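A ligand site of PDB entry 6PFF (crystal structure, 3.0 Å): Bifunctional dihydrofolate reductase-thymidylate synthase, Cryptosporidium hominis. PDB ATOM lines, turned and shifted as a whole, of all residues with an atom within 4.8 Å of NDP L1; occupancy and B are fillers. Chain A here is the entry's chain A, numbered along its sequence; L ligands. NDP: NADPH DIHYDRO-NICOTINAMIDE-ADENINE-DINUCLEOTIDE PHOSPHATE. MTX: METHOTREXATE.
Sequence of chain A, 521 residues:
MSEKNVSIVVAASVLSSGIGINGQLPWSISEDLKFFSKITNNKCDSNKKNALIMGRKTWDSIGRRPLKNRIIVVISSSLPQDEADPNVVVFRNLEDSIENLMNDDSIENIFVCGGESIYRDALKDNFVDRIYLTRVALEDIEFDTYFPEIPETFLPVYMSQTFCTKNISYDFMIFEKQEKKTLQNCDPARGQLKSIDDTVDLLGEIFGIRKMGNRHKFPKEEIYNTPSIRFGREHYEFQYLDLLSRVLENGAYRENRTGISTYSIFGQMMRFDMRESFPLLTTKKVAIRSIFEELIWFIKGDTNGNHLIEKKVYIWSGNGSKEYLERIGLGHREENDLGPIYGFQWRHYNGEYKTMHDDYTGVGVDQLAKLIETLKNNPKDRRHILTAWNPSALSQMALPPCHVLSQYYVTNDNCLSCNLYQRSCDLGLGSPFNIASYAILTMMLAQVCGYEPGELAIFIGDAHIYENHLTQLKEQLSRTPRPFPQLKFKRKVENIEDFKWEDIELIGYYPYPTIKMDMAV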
ATOM      1  N   VAL A   9     -19.318   9.814  24.969  1.00  0.00           N
ATOM      2  CA  VAL A   9     -20.728  10.137  24.772  1.00  0.00           C
ATOM      3  C   VAL A   9     -21.364   8.942  24.084  1.00  0.00           C
ATOM      4  O   VAL A   9     -20.959   8.583  22.967  1.00  0.00           O
ATOM      5  CB  VAL A   9     -20.926  11.417  23.936  1.00  0.00           C
ATOM      6  CG1 VAL A   9     -22.382  11.844  23.980  1.00  0.00           C
ATOM      7  CG2 VAL A   9     -20.026  12.530  24.443  1.00  0.00           C
ATOM      8  N   VAL A  10     -22.356   8.331  24.725  1.00  0.00           N
ATOM      9  CA  VAL A  10     -22.930   7.097  24.200  1.00  0.00           C
ATOM     10  C   VAL A  10     -24.410   7.031  24.555  1.00  0.00           C
ATOM     11  O   VAL A  10     -24.850   7.569  25.572  1.00  0.00           O
ATOM     12  CB  VAL A  10     -22.161   5.862  24.707  1.00  0.00           C
ATOM     13  CG1 VAL A  10     -22.321   5.713  26.226  1.00  0.00           C
ATOM     14  CG2 VAL A  10     -22.622   4.595  23.990  1.00  0.00           C
ATOM     15  N   ALA A  11     -25.172   6.372  23.684  1.00  0.00           N
ATOM     16  CA  ALA A  11     -26.566   6.045  23.938  1.00  0.00           C
ATOM     17  C   ALA A  11     -26.706   4.536  23.833  1.00  0.00           C
ATOM     18  O   ALA A  11     -26.516   3.964  22.760  1.00  0.00           O
ATOM     19  CB  ALA A  11     -27.502   6.751  22.948  1.00  0.00           C
ATOM     20  N   ILE A  19     -25.961  -0.541  21.278  1.00  0.00           N
ATOM     21  CA  ILE A  19     -25.869   0.818  20.758  1.00  0.00           C
ATOM     22  C   ILE A  19     -26.068   0.856  19.246  1.00  0.00           C
ATOM     23  O   ILE A  19     -26.219   1.939  18.657  1.00  0.00           O
ATOM     24  CB  ILE A  19     -24.533   1.469  21.138  1.00  0.00           C
ATOM     25  CG1 ILE A  19     -23.357   0.726  20.491  1.00  0.00           C
ATOM     26  CG2 ILE A  19     -24.361   1.499  22.649  1.00  0.00           C
ATOM     27  CD1 ILE A  19     -22.023   1.413  20.710  1.00  0.00           C
ATOM     28  N   GLY A  20     -26.066  -0.306  18.588  1.00  0.00           N
ATOM     29  CA  GLY A  20     -26.150  -0.314  17.139  1.00  0.00           C
ATOM     30  C   GLY A  20     -26.656  -1.628  16.590  1.00  0.00           C
ATOM     31  O   GLY A  20     -26.647  -2.660  17.263  1.00  0.00           O
ATOM     32  N   ILE A  21     -27.089  -1.569  15.328  1.00  0.00           N
ATOM     33  CA  ILE A  21     -27.559  -2.756  14.601  1.00  0.00           C
ATOM     34  C   ILE A  21     -27.482  -2.499  13.102  1.00  0.00           C
ATOM     35  O   ILE A  21     -28.079  -1.544  12.592  1.00  0.00           O
ATOM     36  CB  ILE A  21     -28.987  -3.142  15.033  1.00  0.00           C
ATOM     37  CG1 ILE A  21     -29.523  -4.257  14.130  1.00  0.00           C
ATOM     38  CG2 ILE A  21     -29.914  -1.942  15.007  1.00  0.00           C
ATOM     39  CD1 ILE A  21     -28.772  -5.556  14.255  1.00  0.00           C
ATOM     40  N   GLY A  23     -25.148  -1.350  11.135  1.00  0.00           N
ATOM     41  CA  GLY A  23     -24.567  -0.081  10.720  1.00  0.00           C
ATOM     42  C   GLY A  23     -25.402   1.142  11.007  1.00  0.00           C
ATOM     43  O   GLY A  23     -25.102   2.215  10.468  1.00  0.00           O
ATOM     44  N   GLN A  24     -26.446   1.035  11.814  1.00  0.00           N
ATOM     45  CA  GLN A  24     -27.275   2.179  12.177  1.00  0.00           C
ATOM     46  C   GLN A  24     -27.699   2.039  13.631  1.00  0.00           C
ATOM     47  O   GLN A  24     -27.363   1.066  14.314  1.00  0.00           O
ATOM     48  CB  GLN A  24     -28.497   2.308  11.263  1.00  0.00           C
ATOM     49  CG  GLN A  24     -29.409   1.101  11.261  1.00  0.00           C
ATOM     50  CD  GLN A  24     -30.640   1.320  10.413  1.00  0.00           C
ATOM     51  OE1 GLN A  24     -30.845   2.399   9.849  1.00  0.00           O
ATOM     52  NE2 GLN A  24     -31.493   0.297  10.325  1.00  0.00           N
ATOM     53  N   LEU A  25     -28.452   3.034  14.100  1.00  0.00           N
ATOM     54  CA  LEU A  25     -28.931   3.021  15.477  1.00  0.00           C
ATOM     55  C   LEU A  25     -30.176   2.150  15.574  1.00  0.00           C
ATOM     56  O   LEU A  25     -30.981   2.083  14.636  1.00  0.00           O
ATOM     57  CB  LEU A  25     -29.267   4.435  15.933  1.00  0.00           C
ATOM     58  CG  LEU A  25     -28.115   5.411  16.181  1.00  0.00           C
ATOM     59  CD1 LEU A  25     -28.671   6.763  16.548  1.00  0.00           C
ATOM     60  CD2 LEU A  25     -27.188   4.891  17.261  1.00  0.00           C
ATOM     61  N   TRP A  27     -32.746   2.812  17.206  1.00  0.00           N
ATOM     62  CA  TRP A  27     -33.857   3.686  17.561  1.00  0.00           C
ATOM     63  C   TRP A  27     -33.697   5.003  16.811  1.00  0.00           C
ATOM     64  O   TRP A  27     -32.684   5.245  16.160  1.00  0.00           O
ATOM     65  CB  TRP A  27     -33.933   3.917  19.071  1.00  0.00           C
ATOM     66  CG  TRP A  27     -32.610   4.293  19.634  1.00  0.00           C
ATOM     67  CD1 TRP A  27     -31.939   5.477  19.455  1.00  0.00           C
ATOM     68  CD2 TRP A  27     -31.776   3.483  20.471  1.00  0.00           C
ATOM     69  NE1 TRP A  27     -30.746   5.443  20.131  1.00  0.00           N
ATOM     70  CE2 TRP A  27     -30.619   4.242  20.764  1.00  0.00           C
ATOM     71  CE3 TRP A  27     -31.895   2.205  21.008  1.00  0.00           C
ATOM     72  CZ2 TRP A  27     -29.589   3.746  21.570  1.00  0.00           C
ATOM     73  CZ3 TRP A  27     -30.868   1.712  21.801  1.00  0.00           C
ATOM     74  CH2 TRP A  27     -29.733   2.480  22.070  1.00  0.00           C
ATOM     75  N   GLY A  55     -14.837   5.893  15.237  1.00  0.00           N
ATOM     76  CA  GLY A  55     -14.321   4.869  14.342  1.00  0.00           C
ATOM     77  C   GLY A  55     -14.788   5.053  12.909  1.00  0.00           C
ATOM     78  O   GLY A  55     -15.622   5.896  12.604  1.00  0.00           O
ATOM     79  N   ARG A  56     -14.244   4.211  12.029  1.00  0.00           N
ATOM     80  CA  ARG A  56     -14.532   4.373  10.608  1.00  0.00           C
ATOM     81  C   ARG A  56     -15.970   4.003  10.269  1.00  0.00           C
ATOM     82  O   ARG A  56     -16.625   4.691   9.478  1.00  0.00           O
ATOM     83  CB  ARG A  56     -13.583   3.525   9.758  1.00  0.00           C
ATOM     84  CG  ARG A  56     -13.590   3.946   8.291  1.00  0.00           C
ATOM     85  CD  ARG A  56     -13.415   2.783   7.341  1.00  0.00           C
ATOM     86  NE  ARG A  56     -14.629   1.973   7.225  1.00  0.00           N
ATOM     87  CZ  ARG A  56     -14.699   0.685   7.536  1.00  0.00           C
ATOM     88  NH1 ARG A  56     -13.631   0.042   7.990  1.00  0.00           N
ATOM     89  NH2 ARG A  56     -15.855   0.030   7.400  1.00  0.00           N
ATOM     90  N   LYS A  57     -16.484   2.912  10.853  1.00  0.00           N
ATOM     91  CA  LYS A  57     -17.864   2.539  10.561  1.00  0.00           C
ATOM     92  C   LYS A  57     -18.838   3.593  11.101  1.00  0.00           C
ATOM     93  O   LYS A  57     -19.851   3.883  10.465  1.00  0.00           O
ATOM     94  CB  LYS A  57     -18.167   1.159  11.139  1.00  0.00           C
ATOM     95  CG  LYS A  57     -17.284   0.056  10.568  1.00  0.00           C
ATOM     96  CD  LYS A  57     -17.687  -1.321  11.070  1.00  0.00           C
ATOM     97  CE  LYS A  57     -16.809  -2.404  10.468  1.00  0.00           C
ATOM     98  NZ  LYS A  57     -17.190  -3.760  10.948  1.00  0.00           N
ATOM     99  N   THR A  58     -18.524   4.171  12.262  1.00  0.00           N
ATOM    100  CA  THR A  58     -19.316   5.287  12.752  1.00  0.00           C
ATOM    101  C   THR A  58     -19.233   6.479  11.811  1.00  0.00           C
ATOM    102  O   THR A  58     -20.244   7.144  11.520  1.00  0.00           O
ATOM    103  CB  THR A  58     -18.846   5.676  14.156  1.00  0.00           C
ATOM    104  OG1 THR A  58     -19.270   4.664  15.088  1.00  0.00           O
ATOM    105  CG2 THR A  58     -19.402   7.011  14.585  1.00  0.00           C
ATOM    106  N   SER A  61     -21.560   5.887   9.227  1.00  0.00           N
ATOM    107  CA  SER A  61     -22.954   5.971   9.666  1.00  0.00           C
ATOM    108  C   SER A  61     -23.498   7.388   9.572  1.00  0.00           C
ATOM    109  O   SER A  61     -24.697   7.575   9.384  1.00  0.00           O
ATOM    110  CB  SER A  61     -23.073   5.464  11.101  1.00  0.00           C
ATOM    111  OG  SER A  61     -22.663   4.109  11.199  1.00  0.00           O
ATOM    112  N   ILE A  75     -10.728   7.319  13.359  1.00  0.00           N
ATOM    113  CA  ILE A  75      -9.739   6.259  13.576  1.00  0.00           C
ATOM    114  C   ILE A  75      -9.941   5.217  12.498  1.00  0.00           C
ATOM    115  O   ILE A  75     -11.013   4.604  12.393  1.00  0.00           O
ATOM    116  CB  ILE A  75      -9.878   5.648  14.982  1.00  0.00           C
ATOM    117  CG1 ILE A  75      -9.780   6.736  16.046  1.00  0.00           C
ATOM    118  CG2 ILE A  75      -8.829   4.572  15.183  1.00  0.00           C
ATOM    119  CD1 ILE A  75      -8.506   7.550  15.981  1.00  0.00           C
ATOM    120  N   SER A  76      -8.914   5.006  11.672  1.00  0.00           N
ATOM    121  CA  SER A  76      -8.988   4.049  10.583  1.00  0.00           C
ATOM    122  C   SER A  76      -7.578   3.727  10.121  1.00  0.00           C
ATOM    123  O   SER A  76      -6.704   4.594  10.125  1.00  0.00           O
ATOM    124  CB  SER A  76      -9.832   4.575   9.421  1.00  0.00           C
ATOM    125  OG  SER A  76      -9.903   3.629   8.363  1.00  0.00           O
ATOM    126  N   SER A  77      -7.375   2.484   9.709  1.00  0.00           N
ATOM    127  CA  SER A  77      -6.099   2.059   9.161  1.00  0.00           C
ATOM    128  C   SER A  77      -6.049   2.147   7.642  1.00  0.00           C
ATOM    129  O   SER A  77      -4.965   2.036   7.064  1.00  0.00           O
ATOM    130  CB  SER A  77      -5.801   0.615   9.585  1.00  0.00           C
ATOM    131  OG  SER A  77      -6.805  -0.257   9.111  1.00  0.00           O
ATOM    132  N   SER A  78      -7.201   2.364   6.986  1.00  0.00           N
ATOM    133  CA  SER A  78      -7.287   2.386   5.536  1.00  0.00           C
ATOM    134  C   SER A  78      -7.666   3.734   4.943  1.00  0.00           C
ATOM    135  O   SER A  78      -7.340   3.983   3.785  1.00  0.00           O
ATOM    136  CB  SER A  78      -8.295   1.336   5.043  1.00  0.00           C
ATOM    137  OG  SER A  78      -9.608   1.635   5.473  1.00  0.00           O
ATOM    138  N   ARG A  92      -4.275   6.642  12.623  1.00  0.00           N
ATOM    139  CA  ARG A  92      -4.154   5.204  12.417  1.00  0.00           C
ATOM    140  C   ARG A  92      -4.522   4.404  13.662  1.00  0.00           C
ATOM    141  O   ARG A  92      -4.907   3.232  13.543  1.00  0.00           O
ATOM    142  CB  ARG A  92      -2.733   4.842  11.974  1.00  0.00           C
ATOM    143  CG  ARG A  92      -2.339   5.454  10.636  1.00  0.00           C
ATOM    144  CD  ARG A  92      -3.329   5.084   9.560  1.00  0.00           C
ATOM    145  NE  ARG A  92      -3.089   5.812   8.324  1.00  0.00           N
ATOM    146  CZ  ARG A  92      -3.888   5.773   7.265  1.00  0.00           C
ATOM    147  NH1 ARG A  92      -4.993   5.047   7.288  1.00  0.00           N
ATOM    148  NH2 ARG A  92      -3.578   6.469   6.170  1.00  0.00           N
ATOM    149  N   ASN A  93      -4.408   4.995  14.850  1.00  0.00           N
ATOM    150  CA  ASN A  93      -4.783   4.315  16.072  1.00  0.00           C
ATOM    151  C   ASN A  93      -5.333   5.340  17.055  1.00  0.00           C
ATOM    152  O   ASN A  93      -5.148   6.551  16.897  1.00  0.00           O
ATOM    153  CB  ASN A  93      -3.604   3.555  16.692  1.00  0.00           C
ATOM    154  CG  ASN A  93      -2.456   4.473  17.060  1.00  0.00           C
ATOM    155  OD1 ASN A  93      -2.344   4.901  18.203  1.00  0.00           O
ATOM    156  ND2 ASN A  93      -1.608   4.778  16.094  1.00  0.00           N
ATOM    157  N   CYS A 113     -16.863   9.219  20.884  1.00  0.00           N
ATOM    158  CA  CYS A 113     -18.242   8.886  20.579  1.00  0.00           C
ATOM    159  C   CYS A 113     -18.340   7.871  19.444  1.00  0.00           C
ATOM    160  O   CYS A 113     -19.403   7.734  18.835  1.00  0.00           O
ATOM    161  CB  CYS A 113     -19.033  10.150  20.246  1.00  0.00           C
ATOM    162  SG  CYS A 113     -18.104  11.368  19.287  1.00  0.00           S
ATOM    163  N   GLY A 114     -17.252   7.143  19.165  1.00  0.00           N
ATOM    164  CA  GLY A 114     -17.214   6.173  18.102  1.00  0.00           C
ATOM    165  C   GLY A 114     -17.981   4.909  18.406  1.00  0.00           C
ATOM    166  O   GLY A 114     -18.903   4.920  19.232  1.00  0.00           O
ATOM    167  N   GLY A 115     -17.623   3.804  17.759  1.00  0.00           N
ATOM    168  CA  GLY A 115     -18.310   2.552  17.932  1.00  0.00           C
ATOM    169  C   GLY A 115     -17.784   1.762  19.115  1.00  0.00           C
ATOM    170  O   GLY A 115     -16.988   2.249  19.925  1.00  0.00           O
ATOM    171  N   GLU A 116     -18.244   0.515  19.208  1.00  0.00           N
ATOM    172  CA  GLU A 116     -17.804  -0.355  20.294  1.00  0.00           C
ATOM    173  C   GLU A 116     -16.298  -0.525  20.293  1.00  0.00           C
ATOM    174  O   GLU A 116     -15.666  -0.547  21.362  1.00  0.00           O
ATOM    175  CB  GLU A 116     -18.504  -1.708  20.179  1.00  0.00           C
ATOM    176  CG  GLU A 116     -17.941  -2.787  21.081  1.00  0.00           C
ATOM    177  CD  GLU A 116     -18.766  -4.051  21.078  1.00  0.00           C
ATOM    178  OE1 GLU A 116     -19.789  -4.083  20.346  1.00  0.00           O
ATOM    179  OE2 GLU A 116     -18.393  -5.006  21.780  1.00  0.00           O
ATOM    180  N   SER A 117     -15.680  -0.643  19.110  1.00  0.00           N
ATOM    181  CA  SER A 117     -14.233  -0.837  19.049  1.00  0.00           C
ATOM    182  C   SER A 117     -13.495   0.345  19.670  1.00  0.00           C
ATOM    183  O   SER A 117     -12.476   0.159  20.330  1.00  0.00           O
ATOM    184  CB  SER A 117     -13.796  -1.061  17.603  1.00  0.00           C
ATOM    185  OG  SER A 117     -14.016   0.084  16.805  1.00  0.00           O
ATOM    186  N   ILE A 118     -13.997   1.557  19.461  1.00  0.00           N
ATOM    187  CA  ILE A 118     -13.333   2.731  20.020  1.00  0.00           C
ATOM    188  C   ILE A 118     -13.601   2.842  21.518  1.00  0.00           C
ATOM    189  O   ILE A 118     -12.682   3.127  22.300  1.00  0.00           O
ATOM    190  CB  ILE A 118     -13.770   4.002  19.272  1.00  0.00           C
ATOM    191  CG1 ILE A 118     -13.423   3.882  17.787  1.00  0.00           C
ATOM    192  CG2 ILE A 118     -13.095   5.232  19.873  1.00  0.00           C
ATOM    193  CD1 ILE A 118     -11.959   3.666  17.525  1.00  0.00           C
ATOM    194  N   TYR A 119     -14.857   2.638  21.944  1.00  0.00           N
ATOM    195  CA  TYR A 119     -15.183   2.712  23.363  1.00  0.00           C
ATOM    196  C   TYR A 119     -14.356   1.714  24.173  1.00  0.00           C
ATOM    197  O   TYR A 119     -13.790   2.053  25.214  1.00  0.00           O
ATOM    198  CB  TYR A 119     -16.671   2.422  23.577  1.00  0.00           C
ATOM    199  CG  TYR A 119     -17.625   3.487  23.089  1.00  0.00           C
ATOM    200  CD1 TYR A 119     -17.319   4.834  23.205  1.00  0.00           C
ATOM    201  CD2 TYR A 119     -18.836   3.129  22.509  1.00  0.00           C
ATOM    202  CE1 TYR A 119     -18.206   5.804  22.755  1.00  0.00           C
ATOM    203  CE2 TYR A 119     -19.719   4.082  22.055  1.00  0.00           C
ATOM    204  CZ  TYR A 119     -19.405   5.420  22.189  1.00  0.00           C
ATOM    205  OH  TYR A 119     -20.295   6.366  21.734  1.00  0.00           O
ATOM    206  N   ASP A 121     -11.464   0.091  23.872  1.00  0.00           N
ATOM    207  CA  ASP A 121     -10.060   0.385  24.155  1.00  0.00           C
ATOM    208  C   ASP A 121      -9.806   1.859  24.444  1.00  0.00           C
ATOM    209  O   ASP A 121      -8.654   2.250  24.636  1.00  0.00           O
ATOM    210  CB  ASP A 121      -9.166  -0.102  23.009  1.00  0.00           C
ATOM    211  CG  ASP A 121      -9.662   0.317  21.652  1.00  0.00           C
ATOM    212  OD1 ASP A 121     -10.318   1.382  21.556  1.00  0.00           O
ATOM    213  OD2 ASP A 121      -9.400  -0.414  20.675  1.00  0.00           O
ATOM    214  N   THR A 145     -23.878  -4.342  18.169  1.00  0.00           N
ATOM    215  CA  THR A 145     -22.803  -3.499  18.683  1.00  0.00           C
ATOM    216  C   THR A 145     -23.216  -3.016  20.059  1.00  0.00           C
ATOM    217  O   THR A 145     -24.311  -2.485  20.234  1.00  0.00           O
ATOM    218  CB  THR A 145     -22.541  -2.315  17.749  1.00  0.00           C
ATOM    219  OG1 THR A 145     -22.132  -2.811  16.466  1.00  0.00           O
ATOM    220  CG2 THR A 145     -21.462  -1.421  18.302  1.00  0.00           C
HETATM  221  PA  NDP L   1     -16.665   1.492  14.717  1.00  0.00           P
HETATM  222  O1A NDP L   1     -15.992   1.265  16.055  1.00  0.00           O
HETATM  223  O2A NDP L   1     -17.457   2.768  14.741  1.00  0.00           O
HETATM  224  O5B NDP L   1     -15.594   1.641  13.634  1.00  0.00           O
HETATM  225  C5B NDP L   1     -14.639   0.632  13.433  1.00  0.00           C
HETATM  226  C4B NDP L   1     -13.512   0.969  12.546  1.00  0.00           C
HETATM  227  O4B NDP L   1     -12.645   1.869  13.216  1.00  0.00           O
HETATM  228  C3B NDP L   1     -12.682  -0.191  12.223  1.00  0.00           C
HETATM  229  O3B NDP L   1     -13.177  -0.862  11.112  1.00  0.00           O
HETATM  230  C2B NDP L   1     -11.404   0.419  11.947  1.00  0.00           C
HETATM  231  O2B NDP L   1     -11.418   1.047  10.700  1.00  0.00           O
HETATM  232  C1B NDP L   1     -11.316   1.463  12.943  1.00  0.00           C
HETATM  233  N9A NDP L   1     -10.675   0.995  14.128  1.00  0.00           N
HETATM  234  C8A NDP L   1     -11.278   0.556  15.251  1.00  0.00           C
HETATM  235  N7A NDP L   1     -10.347   0.194  16.153  1.00  0.00           N
HETATM  236  C5A NDP L   1      -9.112   0.410  15.601  1.00  0.00           C
HETATM  237  C6A NDP L   1      -7.776   0.232  16.045  1.00  0.00           C
HETATM  238  N6A NDP L   1      -7.533  -0.304  17.410  1.00  0.00           N
HETATM  239  N1A NDP L   1      -6.729   0.560  15.231  1.00  0.00           N
HETATM  240  C2A NDP L   1      -6.986   1.048  13.991  1.00  0.00           C
HETATM  241  N3A NDP L   1      -8.225   1.229  13.528  1.00  0.00           N
HETATM  242  C4A NDP L   1      -9.317   0.918  14.318  1.00  0.00           C
HETATM  243  O3  NDP L   1     -17.642   0.280  14.349  1.00  0.00           O
HETATM  244  PN  NDP L   1     -18.646  -0.379  15.389  1.00  0.00           P
HETATM  245  O1N NDP L   1     -19.303  -1.642  14.806  1.00  0.00           O
HETATM  246  O2N NDP L   1     -17.881  -0.776  16.632  1.00  0.00           O
HETATM  247  O5D NDP L   1     -19.792   0.710  15.756  1.00  0.00           O
HETATM  248  C5D NDP L   1     -20.725   1.119  14.792  1.00  0.00           C
HETATM  249  C4D NDP L   1     -22.127   0.882  15.091  1.00  0.00           C
HETATM  250  O4D NDP L   1     -22.433   1.432  16.374  1.00  0.00           O
HETATM  251  C3D NDP L   1     -23.002   1.582  14.139  1.00  0.00           C
HETATM  252  O3D NDP L   1     -24.207   0.903  14.037  1.00  0.00           O
HETATM  253  C2D NDP L   1     -23.225   2.850  14.761  1.00  0.00           C
HETATM  254  O2D NDP L   1     -24.413   3.415  14.297  1.00  0.00           O
HETATM  255  C1D NDP L   1     -23.321   2.475  16.192  1.00  0.00           C
HETATM  256  N1N NDP L   1     -23.018   3.610  17.028  1.00  0.00           N
HETATM  257  C2N NDP L   1     -23.827   3.880  18.069  1.00  0.00           C
HETATM  258  C3N NDP L   1     -23.577   4.968  18.911  1.00  0.00           C
HETATM  259  C7N NDP L   1     -24.518   5.249  20.077  1.00  0.00           C
HETATM  260  O7N NDP L   1     -24.230   6.150  20.876  1.00  0.00           O
HETATM  261  N7N NDP L   1     -25.718   4.497  20.275  1.00  0.00           N
HETATM  262  C4N NDP L   1     -22.465   5.795  18.674  1.00  0.00           C
HETATM  263  C5N NDP L   1     -21.642   5.486  17.584  1.00  0.00           C
HETATM  264  C6N NDP L   1     -21.930   4.392  16.763  1.00  0.00           C
HETATM  265  P2B NDP L   1     -10.657   0.440   9.485  1.00  0.00           P
HETATM  266  O1X NDP L   1     -11.273  -0.944   9.177  1.00  0.00           O
HETATM  267  O2X NDP L   1     -10.815   1.346   8.331  1.00  0.00           O
HETATM  268  O3X NDP L   1      -9.199   0.304   9.782  1.00  0.00           O
HETATM  269  N1  MTX L   2     -26.384   9.436  21.016  1.00  0.00           N
HETATM  270  C2  MTX L   2     -25.633   9.676  22.109  1.00  0.00           C
HETATM  271  NA2 MTX L   2     -26.301  10.008  23.344  1.00  0.00           N
HETATM  272  N3  MTX L   2     -24.296   9.629  22.089  1.00  0.00           N
HETATM  273  C4  MTX L   2     -23.647   9.326  20.937  1.00  0.00           C
HETATM  274  NA4 MTX L   2     -22.218   9.261  20.880  1.00  0.00           N
HETATM  275  C4A MTX L   2     -24.392   9.056  19.777  1.00  0.00           C
HETATM  276  N5  MTX L   2     -23.767   8.734  18.612  1.00  0.00           N
HETATM  277  C6  MTX L   2     -24.518   8.481  17.523  1.00  0.00           C
HETATM  278  C7  MTX L   2     -25.915   8.544  17.537  1.00  0.00           C
HETATM  279  N8  MTX L   2     -26.521   8.860  18.712  1.00  0.00           N
HETATM  280  C8A MTX L   2     -25.768   9.111  19.837  1.00  0.00           C
HETATM  281  C9  MTX L   2     -23.779   8.150  16.259  1.00  0.00           C
HETATM  282  N10 MTX L   2     -23.006   9.301  15.861  1.00  0.00           N
HETATM  283  CM  MTX L   2     -21.568   9.304  15.966  1.00  0.00           C
HETATM  284  C11 MTX L   2     -25.001  12.776  14.559  1.00  0.00           C
HETATM  285  C12 MTX L   2     -25.534  11.535  14.246  1.00  0.00           C
HETATM  286  C13 MTX L   2     -24.875  10.383  14.668  1.00  0.00           C
HETATM  287  C14 MTX L   2     -23.702  10.491  15.411  1.00  0.00           C
HETATM  288  C15 MTX L   2     -23.179  11.742  15.728  1.00  0.00           C
HETATM  289  C16 MTX L   2     -23.835  12.878  15.302  1.00  0.00           C
HETATM  290  C   MTX L   2     -25.667  14.062  14.133  1.00  0.00           C
HETATM  291  O   MTX L   2     -26.328  14.108  13.111  1.00  0.00           O
HETATM  292  N   MTX L   2     -25.490  15.222  14.976  1.00  0.00           N
HETATM  293  CA  MTX L   2     -26.079  16.509  14.683  1.00  0.00           C
HETATM  294  CT  MTX L   2     -25.253  17.503  15.406  1.00  0.00           C
HETATM  295  O1  MTX L   2     -24.439  17.103  16.284  1.00  0.00           O
HETATM  296  O2  MTX L   2     -25.357  18.736  15.146  1.00  0.00           O
HETATM  297  CB  MTX L   2     -27.446  16.504  15.266  1.00  0.00           C
HETATM  298  CG  MTX L   2     -28.389  17.634  14.998  1.00  0.00           C
HETATM  299  CD  MTX L   2     -29.688  17.570  15.731  1.00  0.00           C
HETATM  300  OE1 MTX L   2     -30.077  18.579  16.354  1.00  0.00           O
HETATM  301  OE2 MTX L   2     -30.512  16.653  15.448  1.00  0.00           O
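An oxygen (O4B) of NDP L1 lies close to the backbone carbonyl oxygen (O) of Ile 75 (3.3 Å). Merely in contact with NDP L1: Arg 92, Gly 114, Gly 23, Leu 25, Cys 113, Gly 55, Ser 61, Val 10, Asp 121, Tyr 119, Gly 20 and Ile 118. Hydrophobic or aromatic side chains that line NDP L1: Val 10, Ala 11, Ile 19, Leu 25, Ile 75 and Ile 118. Of the 30 residues printed, 26 come within 4 Å of NDP L1.
O of Ser 76 sits at hydrogen-bond distance from NH1 of Arg 92 (3.3 Å). The side-chain hydroxyl of Ser 76 is in hydrogen-bond range of the backbone NH of Ser 78 (3.3 Å). NH1 of Arg 92 lies within hydrogen-bond range of O of Ser 77 (3.0 Å). OG1 of Thr 58 lies within hydrogen-bond range of N of Gly 115 (3.3 Å). N of Ile 19 lies within hydrogen-bond range of O of Thr 145, 2.8 Å away. OH of Tyr 119 lies close to O of Gly 114. The backbone carbonyl oxygen (O) of Cys 113 lies within hydrogen-bond range of the side-chain hydroxyl (OH) of Tyr 119, at 3.3 Å. OH of Tyr 119 is in hydrogen-bond range of O of Val 9, 2.6 Å away.
O2N of NDP L1 is in hydrogen-bond range of N of Ser 117 (3.3 Å). OG of Ser 117 is in hydrogen-bond range of O1A of NDP L1 (2.4 Å). O2X of NDP L1 lies within hydrogen-bond range of OG of Ser 76 (2.5 Å). The backbone NH (N) of Ser 77 is in hydrogen-bond range of an oxygen (O3X) of NDP L1 (2.8 Å). The side-chain hydroxyl (OG) of Ser 77 is in hydrogen-bond range of an oxygen (O3X) of NDP L1, at 2.5 Å. N of Thr 58 sits at hydrogen-bond distance from O2A of NDP L1 (3.0 Å). The side-chain hydroxyl (OG1) of Thr 58 is in hydrogen-bond range of an oxygen (O2A) of NDP L1, 2.6 Å away. N of Ala 11 is in hydrogen-bond range of O7N of NDP L1, 3.0 Å away. The backbone carbonyl oxygen of Ala 11 is in hydrogen-bond range of a nitrogen (N7N) of NDP L1 (2.7 Å). N of Arg 56 is in hydrogen-bond range of O4B of NDP L1 (3.1 Å). An oxygen (O1X) of NDP L1 is in salt-bridge range of the guanidinium group (NH1) of Arg 56 (2.8 Å). The backbone NH (N) of Glu 116 is in hydrogen-bond range of an oxygen (O2N) of NDP L1, 2.9 Å away. The backbone carbonyl oxygen (O) of Ile 19 is in hydrogen-bond range of a nitrogen (N7N) of NDP L1 (3.1 Å). O2X of NDP L1 sits at hydrogen-bond distance from OG of Ser 78 (3.1 Å). The backbone NH of Gln 24 sits at hydrogen-bond distance from an oxygen (O3D) of NDP L1 (3.2 Å). An oxygen (O3D) of NDP L1 sits at hydrogen-bond distance from the backbone carbonyl oxygen (O) of Gln 24 (3.2 Å). O5B of NDP L1 lies within hydrogen-bond range of N of Lys 57. The backbone NH of Gly 115 sits at hydrogen-bond distance from an oxygen (O2A) of NDP L1 (3.2 Å). The side-chain hydroxyl (OG1) of Thr 145 is in hydrogen-bond range of an oxygen (O1N) of NDP L1 (3.5 Å). NA4 of MTX L2 lies within hydrogen-bond range of O of Val 9 (2.5 Å).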
